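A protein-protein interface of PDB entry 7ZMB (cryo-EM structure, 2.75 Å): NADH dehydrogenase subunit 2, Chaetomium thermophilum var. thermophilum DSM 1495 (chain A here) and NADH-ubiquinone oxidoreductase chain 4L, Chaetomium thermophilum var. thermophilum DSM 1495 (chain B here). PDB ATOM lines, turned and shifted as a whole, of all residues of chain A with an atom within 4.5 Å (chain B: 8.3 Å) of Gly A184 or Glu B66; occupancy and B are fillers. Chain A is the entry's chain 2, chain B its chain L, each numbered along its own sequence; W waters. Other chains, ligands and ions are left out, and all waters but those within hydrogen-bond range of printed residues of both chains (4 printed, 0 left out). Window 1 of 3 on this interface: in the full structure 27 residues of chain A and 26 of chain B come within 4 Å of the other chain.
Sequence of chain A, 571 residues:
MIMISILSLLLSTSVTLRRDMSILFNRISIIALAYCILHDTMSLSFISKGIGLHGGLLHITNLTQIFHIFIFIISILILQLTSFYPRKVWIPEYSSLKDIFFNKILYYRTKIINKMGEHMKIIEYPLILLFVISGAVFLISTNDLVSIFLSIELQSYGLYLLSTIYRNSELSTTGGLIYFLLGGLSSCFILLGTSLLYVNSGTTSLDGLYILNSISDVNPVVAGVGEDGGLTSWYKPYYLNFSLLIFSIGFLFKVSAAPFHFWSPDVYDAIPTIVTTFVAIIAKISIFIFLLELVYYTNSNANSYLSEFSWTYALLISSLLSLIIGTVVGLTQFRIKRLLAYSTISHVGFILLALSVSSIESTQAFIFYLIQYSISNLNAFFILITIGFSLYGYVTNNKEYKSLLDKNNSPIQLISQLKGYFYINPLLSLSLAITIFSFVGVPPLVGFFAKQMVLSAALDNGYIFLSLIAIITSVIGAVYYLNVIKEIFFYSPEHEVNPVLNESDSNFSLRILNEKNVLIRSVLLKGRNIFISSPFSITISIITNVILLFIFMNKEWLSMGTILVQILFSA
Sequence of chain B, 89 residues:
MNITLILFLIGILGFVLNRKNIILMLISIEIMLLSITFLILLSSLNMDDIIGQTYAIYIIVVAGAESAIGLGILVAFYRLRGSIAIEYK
The side-chain hydroxyl (OH) of Tyr A157 is in hydrogen-bond range of the backbone carbonyl oxygen (O) of Val B62 (3.5 Å).
The backbone NH (N) of Ile B12 sits close to the side-chain sulfur (SD) of Met B32 (3.8 Å).
The side-chain sulfur of Cys A188 lies within hydrogen-bond range of the backbone carbonyl oxygen of Gly A184 (3.6 Å).
Among the printed residues, pairs that only touch across the chains: Tyr A157 with Glu B66 (2.9 Å), Tyr A160 with Ile B73 (3.9 Å), Phe A180 with Glu B66 (3.1 Å), Phe A180 with Ile B69 (3.9 Å), Phe A180 with Gly B70 (3.3 Å), Leu A181 with Phe B15 (3.3 Å), Gly A184 with Glu B66 (3.5 Å), Leu A185 with Ile B12 (3.5 Å), Leu A185 with Phe B15 (3.7 Å), Cys A188 with Met B32 (3.8 Å) and Cys A188 with Leu B33 (3.8 Å).
Of chain B, only Glu B66 (3.5 Å) comes within 4 Å of Gly A184.
Glu B66 touches just these residues of chain A: Tyr A157 (2.9 Å), Phe A180 (3.1 Å) and Gly A184 (3.5 Å).
No residue of chain B comes within 4 Å of Gly A183.
Of the printed residues of chain A, Leu B33 touches Cys A188 (3.8 Å).
Of the printed residues of chain A, Phe B15 touches Leu A181 (3.3 Å) and Leu A185 (3.7 Å).
Printed residues of chain A within 4 Å of Ile B73: Tyr A160 (3.9 Å).
Met B25 touches none of the printed residues of chain A.
The nearest residue of chain B that does not touch Gly A184 is Ile B29 (4.3 Å).
The nearest printed residue of chain A that does not touch Met B32 is Leu A185 (4.4 Å).
Of the 24 printed residues of chain B, 9 touch a printed residue of chain A.
Printed residues of chain B that touch a printed residue of chain A: Ile B12, Phe B15, Met B32, Leu B33, Val B62, Glu B66, Ile B69, Gly B70 and Ile B73.
Hydrophobic or aromatic side chains of chain B within 4 Å of the printed part of chain A: Ile B12, Phe B15, Met B32, Leu B33, Ile B69 and Ile B73.
Printed residues of chain A that touch a printed residue of chain B: Tyr A157, Tyr A160, Phe A180, Leu A181, Gly A184, Leu A185 and Cys A188.
Hydrophobic or aromatic side chains of chain A within 4 Å of the printed part of chain B: Tyr A157, Tyr A160, Phe A180 and Leu A185.
Among the printed residues, no Asp or Glu carboxylate lies within 4 Å of a Lys or Arg side-chain nitrogen of the other chain.
Water W2 lies within hydrogen-bond range of the side-chain carboxylate (OE2) of Glu B66 and the backbone carbonyl oxygen (O) of Phe A180.
Water W3 lies within hydrogen-bond range of O of Gly A184 (3.0 Å), OE1 of Glu B66 (3.5 Å) and SG of Cys A188 (3.5 Å).
Water W1 lies within hydrogen-bond range of the side-chain carboxylate of Glu B66, the side-chain hydroxyl of Tyr A157 and the side-chain hydroxyl of Ser A187.
Water W4 lies within hydrogen-bond range of OH of Tyr A157 (3.3 Å), OE1 of Glu B66 (3.5 Å) and O of Val B62 (3.5 Å).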
ATOM      1  N   TYR A 157      -2.124 -10.207  32.191  1.00  0.00           N
ATOM      2  CA  TYR A 157      -1.474 -11.509  32.240  1.00  0.00           C
ATOM      3  C   TYR A 157      -2.469 -12.594  32.616  1.00  0.00           C
ATOM      4  O   TYR A 157      -2.431 -13.700  32.067  1.00  0.00           O
ATOM      5  CB  TYR A 157      -0.324 -11.470  33.240  1.00  0.00           C
ATOM      6  CG  TYR A 157       0.849 -10.675  32.744  1.00  0.00           C
ATOM      7  CD1 TYR A 157       1.048 -10.478  31.395  1.00  0.00           C
ATOM      8  CD2 TYR A 157       1.716 -10.060  33.632  1.00  0.00           C
ATOM      9  CE1 TYR A 157       2.089  -9.726  30.937  1.00  0.00           C
ATOM     10  CE2 TYR A 157       2.771  -9.309  33.182  1.00  0.00           C
ATOM     11  CZ  TYR A 157       2.948  -9.143  31.833  1.00  0.00           C
ATOM     12  OH  TYR A 157       3.991  -8.384  31.365  1.00  0.00           O
ATOM     13  N   TYR A 160      -4.453 -13.534  29.676  1.00  0.00           N
ATOM     14  CA  TYR A 160      -3.722 -14.447  28.803  1.00  0.00           C
ATOM     15  C   TYR A 160      -3.775 -15.871  29.333  1.00  0.00           C
ATOM     16  O   TYR A 160      -3.892 -16.821  28.554  1.00  0.00           O
ATOM     17  CB  TYR A 160      -2.264 -14.011  28.642  1.00  0.00           C
ATOM     18  CG  TYR A 160      -2.059 -12.571  28.262  1.00  0.00           C
ATOM     19  CD1 TYR A 160      -2.947 -11.913  27.425  1.00  0.00           C
ATOM     20  CD2 TYR A 160      -0.957 -11.872  28.722  1.00  0.00           C
ATOM     21  CE1 TYR A 160      -2.747 -10.606  27.075  1.00  0.00           C
ATOM     22  CE2 TYR A 160      -0.751 -10.566  28.375  1.00  0.00           C
ATOM     23  CZ  TYR A 160      -1.647  -9.937  27.557  1.00  0.00           C
ATOM     24  OH  TYR A 160      -1.435  -8.629  27.222  1.00  0.00           O
ATOM     25  N   PHE A 180      -1.707 -12.854  24.042  1.00  0.00           N
ATOM     26  CA  PHE A 180      -0.509 -12.523  24.811  1.00  0.00           C
ATOM     27  C   PHE A 180       0.465 -11.700  23.983  1.00  0.00           C
ATOM     28  O   PHE A 180       1.044 -10.729  24.478  1.00  0.00           O
ATOM     29  CB  PHE A 180       0.180 -13.796  25.324  1.00  0.00           C
ATOM     30  CG  PHE A 180       1.539 -13.551  25.937  1.00  0.00           C
ATOM     31  CD1 PHE A 180       2.680 -13.494  25.149  1.00  0.00           C
ATOM     32  CD2 PHE A 180       1.673 -13.374  27.295  1.00  0.00           C
ATOM     33  CE1 PHE A 180       3.901 -13.249  25.698  1.00  0.00           C
ATOM     34  CE2 PHE A 180       2.901 -13.132  27.852  1.00  0.00           C
ATOM     35  CZ  PHE A 180       4.016 -13.063  27.048  1.00  0.00           C
ATOM     36  N   LEU A 181       0.669 -12.085  22.722  1.00  0.00           N
ATOM     37  CA  LEU A 181       1.647 -11.403  21.882  1.00  0.00           C
ATOM     38  C   LEU A 181       1.220  -9.978  21.568  1.00  0.00           C
ATOM     39  O   LEU A 181       1.993  -9.036  21.748  1.00  0.00           O
ATOM     40  CB  LEU A 181       1.869 -12.197  20.599  1.00  0.00           C
ATOM     41  CG  LEU A 181       2.933 -13.293  20.695  1.00  0.00           C
ATOM     42  CD1 LEU A 181       3.151 -13.954  19.362  1.00  0.00           C
ATOM     43  CD2 LEU A 181       4.241 -12.748  21.241  1.00  0.00           C
ATOM     44  N   LEU A 182      -0.011  -9.796  21.097  1.00  0.00           N
ATOM     45  CA  LEU A 182      -0.443  -8.470  20.682  1.00  0.00           C
ATOM     46  C   LEU A 182      -0.762  -7.581  21.870  1.00  0.00           C
ATOM     47  O   LEU A 182      -0.682  -6.354  21.757  1.00  0.00           O
ATOM     48  CB  LEU A 182      -1.650  -8.574  19.762  1.00  0.00           C
ATOM     49  CG  LEU A 182      -1.419  -9.075  18.346  1.00  0.00           C
ATOM     50  CD1 LEU A 182      -2.731  -9.039  17.610  1.00  0.00           C
ATOM     51  CD2 LEU A 182      -0.362  -8.265  17.623  1.00  0.00           C
ATOM     52  N   GLY A 183      -1.135  -8.169  23.005  1.00  0.00           N
ATOM     53  CA  GLY A 183      -1.262  -7.391  24.217  1.00  0.00           C
ATOM     54  C   GLY A 183       0.075  -6.972  24.788  1.00  0.00           C
ATOM     55  O   GLY A 183       0.172  -5.934  25.448  1.00  0.00           O
ATOM     56  N   GLY A 184       1.115  -7.777  24.567  1.00  0.00           N
ATOM     57  CA  GLY A 184       2.451  -7.363  24.948  1.00  0.00           C
ATOM     58  C   GLY A 184       2.935  -6.185  24.131  1.00  0.00           C
ATOM     59  O   GLY A 184       3.632  -5.306  24.640  1.00  0.00           O
ATOM     60  N   LEU A 185       2.575  -6.155  22.850  1.00  0.00           N
ATOM     61  CA  LEU A 185       2.773  -4.949  22.061  1.00  0.00           C
ATOM     62  C   LEU A 185       1.983  -3.786  22.643  1.00  0.00           C
ATOM     63  O   LEU A 185       2.459  -2.648  22.663  1.00  0.00           O
ATOM     64  CB  LEU A 185       2.367  -5.201  20.614  1.00  0.00           C
ATOM     65  CG  LEU A 185       2.572  -4.002  19.694  1.00  0.00           C
ATOM     66  CD1 LEU A 185       4.024  -3.598  19.729  1.00  0.00           C
ATOM     67  CD2 LEU A 185       2.110  -4.307  18.278  1.00  0.00           C
ATOM     68  N   SER A 186       0.763  -4.059  23.111  1.00  0.00           N
ATOM     69  CA  SER A 186      -0.074  -3.019  23.693  1.00  0.00           C
ATOM     70  C   SER A 186       0.554  -2.445  24.954  1.00  0.00           C
ATOM     71  O   SER A 186       0.477  -1.237  25.205  1.00  0.00           O
ATOM     72  CB  SER A 186      -1.464  -3.586  23.986  1.00  0.00           C
ATOM     73  OG  SER A 186      -2.239  -2.710  24.780  1.00  0.00           O
ATOM     74  N   SER A 187       1.176  -3.296  25.763  1.00  0.00           N
ATOM     75  CA  SER A 187       1.768  -2.829  27.008  1.00  0.00           C
ATOM     76  C   SER A 187       3.046  -2.037  26.768  1.00  0.00           C
ATOM     77  O   SER A 187       3.362  -1.132  27.543  1.00  0.00           O
ATOM     78  CB  SER A 187       2.025  -4.012  27.927  1.00  0.00           C
ATOM     79  OG  SER A 187       0.800  -4.543  28.388  1.00  0.00           O
ATOM     80  N   CYS A 188       3.789  -2.363  25.713  1.00  0.00           N
ATOM     81  CA  CYS A 188       4.978  -1.591  25.384  1.00  0.00           C
ATOM     82  C   CYS A 188       4.620  -0.167  24.990  1.00  0.00           C
ATOM     83  O   CYS A 188       5.433   0.745  25.165  1.00  0.00           O
ATOM     84  CB  CYS A 188       5.761  -2.276  24.262  1.00  0.00           C
ATOM     85  SG  CYS A 188       6.783  -3.649  24.783  1.00  0.00           S
ATOM     86  N   ILE B  12      10.627  -2.994  17.963  1.00  0.00           N
ATOM     87  CA  ILE B  12       9.298  -2.847  17.392  1.00  0.00           C
ATOM     88  C   ILE B  12       9.233  -3.530  16.031  1.00  0.00           C
ATOM     89  O   ILE B  12       8.281  -4.262  15.737  1.00  0.00           O
ATOM     90  CB  ILE B  12       8.892  -1.360  17.334  1.00  0.00           C
ATOM     91  CG1 ILE B  12       7.407  -1.228  17.049  1.00  0.00           C
ATOM     92  CG2 ILE B  12       9.627  -0.602  16.265  1.00  0.00           C
ATOM     93  CD1 ILE B  12       6.574  -1.754  18.154  1.00  0.00           C
ATOM     94  N   PHE B  15       9.549  -7.271  16.147  1.00  0.00           N
ATOM     95  CA  PHE B  15       8.265  -7.843  16.521  1.00  0.00           C
ATOM     96  C   PHE B  15       7.295  -7.838  15.349  1.00  0.00           C
ATOM     97  O   PHE B  15       6.612  -8.833  15.103  1.00  0.00           O
ATOM     98  CB  PHE B  15       7.681  -7.062  17.702  1.00  0.00           C
ATOM     99  CG  PHE B  15       6.378  -7.591  18.205  1.00  0.00           C
ATOM    100  CD1 PHE B  15       6.344  -8.644  19.110  1.00  0.00           C
ATOM    101  CD2 PHE B  15       5.180  -7.038  17.778  1.00  0.00           C
ATOM    102  CE1 PHE B  15       5.146  -9.138  19.582  1.00  0.00           C
ATOM    103  CE2 PHE B  15       3.977  -7.529  18.239  1.00  0.00           C
ATOM    104  CZ  PHE B  15       3.960  -8.581  19.146  1.00  0.00           C
ATOM    105  N   MET B  25       9.581 -13.255  18.323  1.00  0.00           N
ATOM    106  CA  MET B  25       8.526 -12.321  18.702  1.00  0.00           C
ATOM    107  C   MET B  25       8.679 -11.913  20.158  1.00  0.00           C
ATOM    108  O   MET B  25       8.737 -10.725  20.490  1.00  0.00           O
ATOM    109  CB  MET B  25       7.166 -12.981  18.485  1.00  0.00           C
ATOM    110  CG  MET B  25       6.805 -13.290  17.056  1.00  0.00           C
ATOM    111  SD  MET B  25       6.699 -11.850  16.017  1.00  0.00           S
ATOM    112  CE  MET B  25       5.222 -11.114  16.705  1.00  0.00           C
ATOM    113  N   LEU B  26       8.772 -12.907  21.036  1.00  0.00           N
ATOM    114  CA  LEU B  26       8.851 -12.694  22.472  1.00  0.00           C
ATOM    115  C   LEU B  26      10.175 -12.056  22.883  1.00  0.00           C
ATOM    116  O   LEU B  26      10.234 -11.362  23.902  1.00  0.00           O
ATOM    117  CB  LEU B  26       8.616 -14.039  23.155  1.00  0.00           C
ATOM    118  CG  LEU B  26       8.918 -14.388  24.600  1.00  0.00           C
ATOM    119  CD1 LEU B  26       7.965 -13.705  25.553  1.00  0.00           C
ATOM    120  CD2 LEU B  26       8.819 -15.888  24.728  1.00  0.00           C
ATOM    121  N   SER B  28      11.681  -9.732  20.979  1.00  0.00           N
ATOM    122  CA  SER B  28      11.631  -8.329  20.585  1.00  0.00           C
ATOM    123  C   SER B  28      10.860  -7.483  21.586  1.00  0.00           C
ATOM    124  O   SER B  28      11.148  -6.291  21.732  1.00  0.00           O
ATOM    125  CB  SER B  28      11.024  -8.203  19.197  1.00  0.00           C
ATOM    126  OG  SER B  28      11.861  -8.837  18.259  1.00  0.00           O
ATOM    127  N   ILE B  29       9.880  -8.066  22.273  1.00  0.00           N
ATOM    128  CA  ILE B  29       9.254  -7.362  23.386  1.00  0.00           C
ATOM    129  C   ILE B  29      10.288  -7.071  24.461  1.00  0.00           C
ATOM    130  O   ILE B  29      10.348  -5.963  25.005  1.00  0.00           O
ATOM    131  CB  ILE B  29       8.074  -8.179  23.937  1.00  0.00           C
ATOM    132  CG1 ILE B  29       6.839  -7.990  23.055  1.00  0.00           C
ATOM    133  CG2 ILE B  29       7.780  -7.795  25.373  1.00  0.00           C
ATOM    134  CD1 ILE B  29       5.891  -9.167  23.078  1.00  0.00           C
ATOM    135  N   GLU B  30      11.140  -8.058  24.742  1.00  0.00           N
ATOM    136  CA  GLU B  30      12.203  -7.918  25.759  1.00  0.00           C
ATOM    137  C   GLU B  30      13.154  -6.782  25.376  1.00  0.00           C
ATOM    138  O   GLU B  30      13.677  -6.139  26.283  1.00  0.00           O
ATOM    139  CB  GLU B  30      12.970  -9.230  25.848  1.00  0.00           C
ATOM    140  CG  GLU B  30      12.150 -10.430  26.271  1.00  0.00           C
ATOM    141  CD  GLU B  30      12.977 -11.699  26.385  1.00  0.00           C
ATOM    142  OE1 GLU B  30      14.220 -11.598  26.314  1.00  0.00           O
ATOM    143  OE2 GLU B  30      12.380 -12.784  26.535  1.00  0.00           O
ATOM    144  N   MET B  32      12.269  -4.024  23.538  1.00  0.00           N
ATOM    145  CA  MET B  32      11.544  -2.735  23.659  1.00  0.00           C
ATOM    146  C   MET B  32      11.535  -2.304  25.127  1.00  0.00           C
ATOM    147  O   MET B  32      11.850  -1.136  25.397  1.00  0.00           O
ATOM    148  CB  MET B  32      10.120  -2.833  23.112  1.00  0.00           C
ATOM    149  CG  MET B  32      10.070  -2.859  21.613  1.00  0.00           C
ATOM    150  SD  MET B  32       8.388  -2.912  20.985  1.00  0.00           S
ATOM    151  CE  MET B  32       8.014  -4.654  21.158  1.00  0.00           C
ATOM    152  N   LEU B  33      11.173  -3.216  26.026  1.00  0.00           N
ATOM    153  CA  LEU B  33      11.126  -2.911  27.474  1.00  0.00           C
ATOM    154  C   LEU B  33      12.512  -2.477  27.935  1.00  0.00           C
ATOM    155  O   LEU B  33      12.582  -1.556  28.751  1.00  0.00           O
ATOM    156  CB  LEU B  33      10.679  -4.168  28.221  1.00  0.00           C
ATOM    157  CG  LEU B  33       9.266  -4.654  27.892  1.00  0.00           C
ATOM    158  CD1 LEU B  33       8.974  -5.991  28.545  1.00  0.00           C
ATOM    159  CD2 LEU B  33       8.230  -3.626  28.297  1.00  0.00           C
ATOM    160  N   ILE B  59      10.199  -2.779  36.251  1.00  0.00           N
ATOM    161  CA  ILE B  59       9.899  -3.151  34.837  1.00  0.00           C
ATOM    162  C   ILE B  59      10.721  -4.392  34.507  1.00  0.00           C
ATOM    163  O   ILE B  59      10.239  -5.204  33.718  1.00  0.00           O
ATOM    164  CB  ILE B  59      10.187  -1.995  33.864  1.00  0.00           C
ATOM    165  CG1 ILE B  59       9.286  -0.786  34.117  1.00  0.00           C
ATOM    166  CG2 ILE B  59      10.125  -2.458  32.417  1.00  0.00           C
ATOM    167  CD1 ILE B  59       9.853   0.497  33.575  1.00  0.00           C
ATOM    168  N   ILE B  60      11.852  -4.594  35.176  1.00  0.00           N
ATOM    169  CA  ILE B  60      12.610  -5.860  34.987  1.00  0.00           C
ATOM    170  C   ILE B  60      11.802  -7.030  35.559  1.00  0.00           C
ATOM    171  O   ILE B  60      11.731  -8.066  34.884  1.00  0.00           O
ATOM    172  CB  ILE B  60      14.037  -5.751  35.568  1.00  0.00           C
ATOM    173  CG1 ILE B  60      14.831  -4.632  34.891  1.00  0.00           C
ATOM    174  CG2 ILE B  60      14.765  -7.082  35.492  1.00  0.00           C
ATOM    175  CD1 ILE B  60      15.946  -4.074  35.737  1.00  0.00           C
ATOM    176  N   VAL B  61      11.196  -6.865  36.735  1.00  0.00           N
ATOM    177  CA  VAL B  61      10.470  -7.997  37.400  1.00  0.00           C
ATOM    178  C   VAL B  61       9.228  -8.377  36.595  1.00  0.00           C
ATOM    179  O   VAL B  61       8.974  -9.582  36.468  1.00  0.00           O
ATOM    180  CB  VAL B  61      10.142  -7.766  38.897  1.00  0.00           C
ATOM    181  CG1 VAL B  61       8.962  -6.835  39.118  1.00  0.00           C
ATOM    182  CG2 VAL B  61       9.928  -9.059  39.651  1.00  0.00           C
ATOM    183  N   VAL B  62       8.512  -7.405  36.046  1.00  0.00           N
ATOM    184  CA  VAL B  62       7.341  -7.730  35.239  1.00  0.00           C
ATOM    185  C   VAL B  62       7.734  -8.141  33.827  1.00  0.00           C
ATOM    186  O   VAL B  62       6.964  -8.814  33.139  1.00  0.00           O
ATOM    187  CB  VAL B  62       6.354  -6.553  35.208  1.00  0.00           C
ATOM    188  CG1 VAL B  62       5.967  -6.134  36.630  1.00  0.00           C
ATOM    189  CG2 VAL B  62       6.947  -5.416  34.444  1.00  0.00           C
ATOM    190  N   ALA B  63       8.914  -7.744  33.359  1.00  0.00           N
ATOM    191  CA  ALA B  63       9.355  -8.190  32.045  1.00  0.00           C
ATOM    192  C   ALA B  63       9.781  -9.648  32.078  1.00  0.00           C
ATOM    193  O   ALA B  63       9.755 -10.324  31.046  1.00  0.00           O
ATOM    194  CB  ALA B  63      10.497  -7.307  31.537  1.00  0.00           C
ATOM    195  N   GLY B  64      10.186 -10.139  33.244  1.00  0.00           N
ATOM    196  CA  GLY B  64      10.505 -11.537  33.416  1.00  0.00           C
ATOM    197  C   GLY B  64       9.259 -12.350  33.661  1.00  0.00           C
ATOM    198  O   GLY B  64       9.164 -13.494  33.216  1.00  0.00           O
ATOM    199  N   ALA B  65       8.295 -11.764  34.370  1.00  0.00           N
ATOM    200  CA  ALA B  65       7.000 -12.412  34.529  1.00  0.00           C
ATOM    201  C   ALA B  65       6.310 -12.591  33.183  1.00  0.00           C
ATOM    202  O   ALA B  65       5.711 -13.638  32.917  1.00  0.00           O
ATOM    203  CB  ALA B  65       6.122 -11.606  35.481  1.00  0.00           C
ATOM    204  N   GLU B  66       6.388 -11.576  32.322  1.00  0.00           N
ATOM    205  CA  GLU B  66       5.806 -11.692  30.991  1.00  0.00           C
ATOM    206  C   GLU B  66       6.490 -12.785  30.180  1.00  0.00           C
ATOM    207  O   GLU B  66       5.819 -13.574  29.506  1.00  0.00           O
ATOM    208  CB  GLU B  66       5.889 -10.353  30.260  1.00  0.00           C
ATOM    209  CG  GLU B  66       5.467 -10.423  28.805  1.00  0.00           C
ATOM    210  CD  GLU B  66       5.585  -9.100  28.088  1.00  0.00           C
ATOM    211  OE1 GLU B  66       6.470  -8.302  28.453  1.00  0.00           O
ATOM    212  OE2 GLU B  66       4.787  -8.855  27.162  1.00  0.00           O
ATOM    213  N   SER B  67       7.819 -12.858  30.237  1.00  0.00           N
ATOM    214  CA  SER B  67       8.535 -13.840  29.429  1.00  0.00           C
ATOM    215  C   SER B  67       8.366 -15.261  29.948  1.00  0.00           C
ATOM    216  O   SER B  67       8.498 -16.209  29.170  1.00  0.00           O
ATOM    217  CB  SER B  67      10.018 -13.479  29.339  1.00  0.00           C
ATOM    218  OG  SER B  67      10.622 -13.423  30.616  1.00  0.00           O
ATOM    219  N   ALA B  68       8.077 -15.434  31.236  1.00  0.00           N
ATOM    220  CA  ALA B  68       7.733 -16.759  31.737  1.00  0.00           C
ATOM    221  C   ALA B  68       6.324 -17.158  31.318  1.00  0.00           C
ATOM    222  O   ALA B  68       6.093 -18.299  30.905  1.00  0.00           O
ATOM    223  CB  ALA B  68       7.879 -16.802  33.255  1.00  0.00           C
ATOM    224  N   ILE B  69       5.370 -16.232  31.406  1.00  0.00           N
ATOM    225  CA  ILE B  69       4.014 -16.523  30.954  1.00  0.00           C
ATOM    226  C   ILE B  69       4.003 -16.759  29.452  1.00  0.00           C
ATOM    227  O   ILE B  69       3.258 -17.605  28.947  1.00  0.00           O
ATOM    228  CB  ILE B  69       3.053 -15.392  31.372  1.00  0.00           C
ATOM    229  CG1 ILE B  69       2.857 -15.408  32.884  1.00  0.00           C
ATOM    230  CG2 ILE B  69       1.700 -15.546  30.698  1.00  0.00           C
ATOM    231  CD1 ILE B  69       2.566 -16.778  33.437  1.00  0.00           C
ATOM    232  N   GLY B  70       4.838 -16.027  28.715  1.00  0.00           N
ATOM    233  CA  GLY B  70       4.937 -16.261  27.287  1.00  0.00           C
ATOM    234  C   GLY B  70       5.496 -17.629  26.953  1.00  0.00           C
ATOM    235  O   GLY B  70       4.914 -18.372  26.164  1.00  0.00           O
ATOM    236  N   LEU B  71       6.631 -17.986  27.558  1.00  0.00           N
ATOM    237  CA  LEU B  71       7.227 -19.284  27.267  1.00  0.00           C
ATOM    238  C   LEU B  71       6.316 -20.423  27.696  1.00  0.00           C
ATOM    239  O   LEU B  71       6.295 -21.475  27.048  1.00  0.00           O
ATOM    240  CB  LEU B  71       8.600 -19.408  27.933  1.00  0.00           C
ATOM    241  CG  LEU B  71       9.728 -18.612  27.277  1.00  0.00           C
ATOM    242  CD1 LEU B  71      10.963 -18.639  28.124  1.00  0.00           C
ATOM    243  CD2 LEU B  71      10.029 -19.146  25.890  1.00  0.00           C
ATOM    244  N   GLY B  72       5.560 -20.233  28.775  1.00  0.00           N
ATOM    245  CA  GLY B  72       4.583 -21.236  29.167  1.00  0.00           C
ATOM    246  C   GLY B  72       3.458 -21.389  28.161  1.00  0.00           C
ATOM    247  O   GLY B  72       3.034 -22.506  27.860  1.00  0.00           O
ATOM    248  N   ILE B  73       2.952 -20.274  27.638  1.00  0.00           N
ATOM    249  CA  ILE B  73       1.892 -20.339  26.640  1.00  0.00           C
ATOM    250  C   ILE B  73       2.430 -20.889  25.331  1.00  0.00           C
ATOM    251  O   ILE B  73       1.751 -21.648  24.629  1.00  0.00           O
ATOM    252  CB  ILE B  73       1.241 -18.956  26.462  1.00  0.00           C
ATOM    253  CG1 ILE B  73       0.308 -18.665  27.636  1.00  0.00           C
ATOM    254  CG2 ILE B  73       0.464 -18.890  25.160  1.00  0.00           C
ATOM    255  CD1 ILE B  73      -0.131 -17.237  27.746  1.00  0.00           C
HETATM  256  O   HOH W   1       2.770  -7.041  28.771  1.00  0.00           O
HETATM  257  O   HOH W   2       2.505 -10.134  27.272  1.00  0.00           O
HETATM  258  O   HOH W   3       5.016  -5.389  27.286  1.00  0.00           O
HETATM  259  O   HOH W   4       6.260  -6.058  31.117  1.00  0.00           O
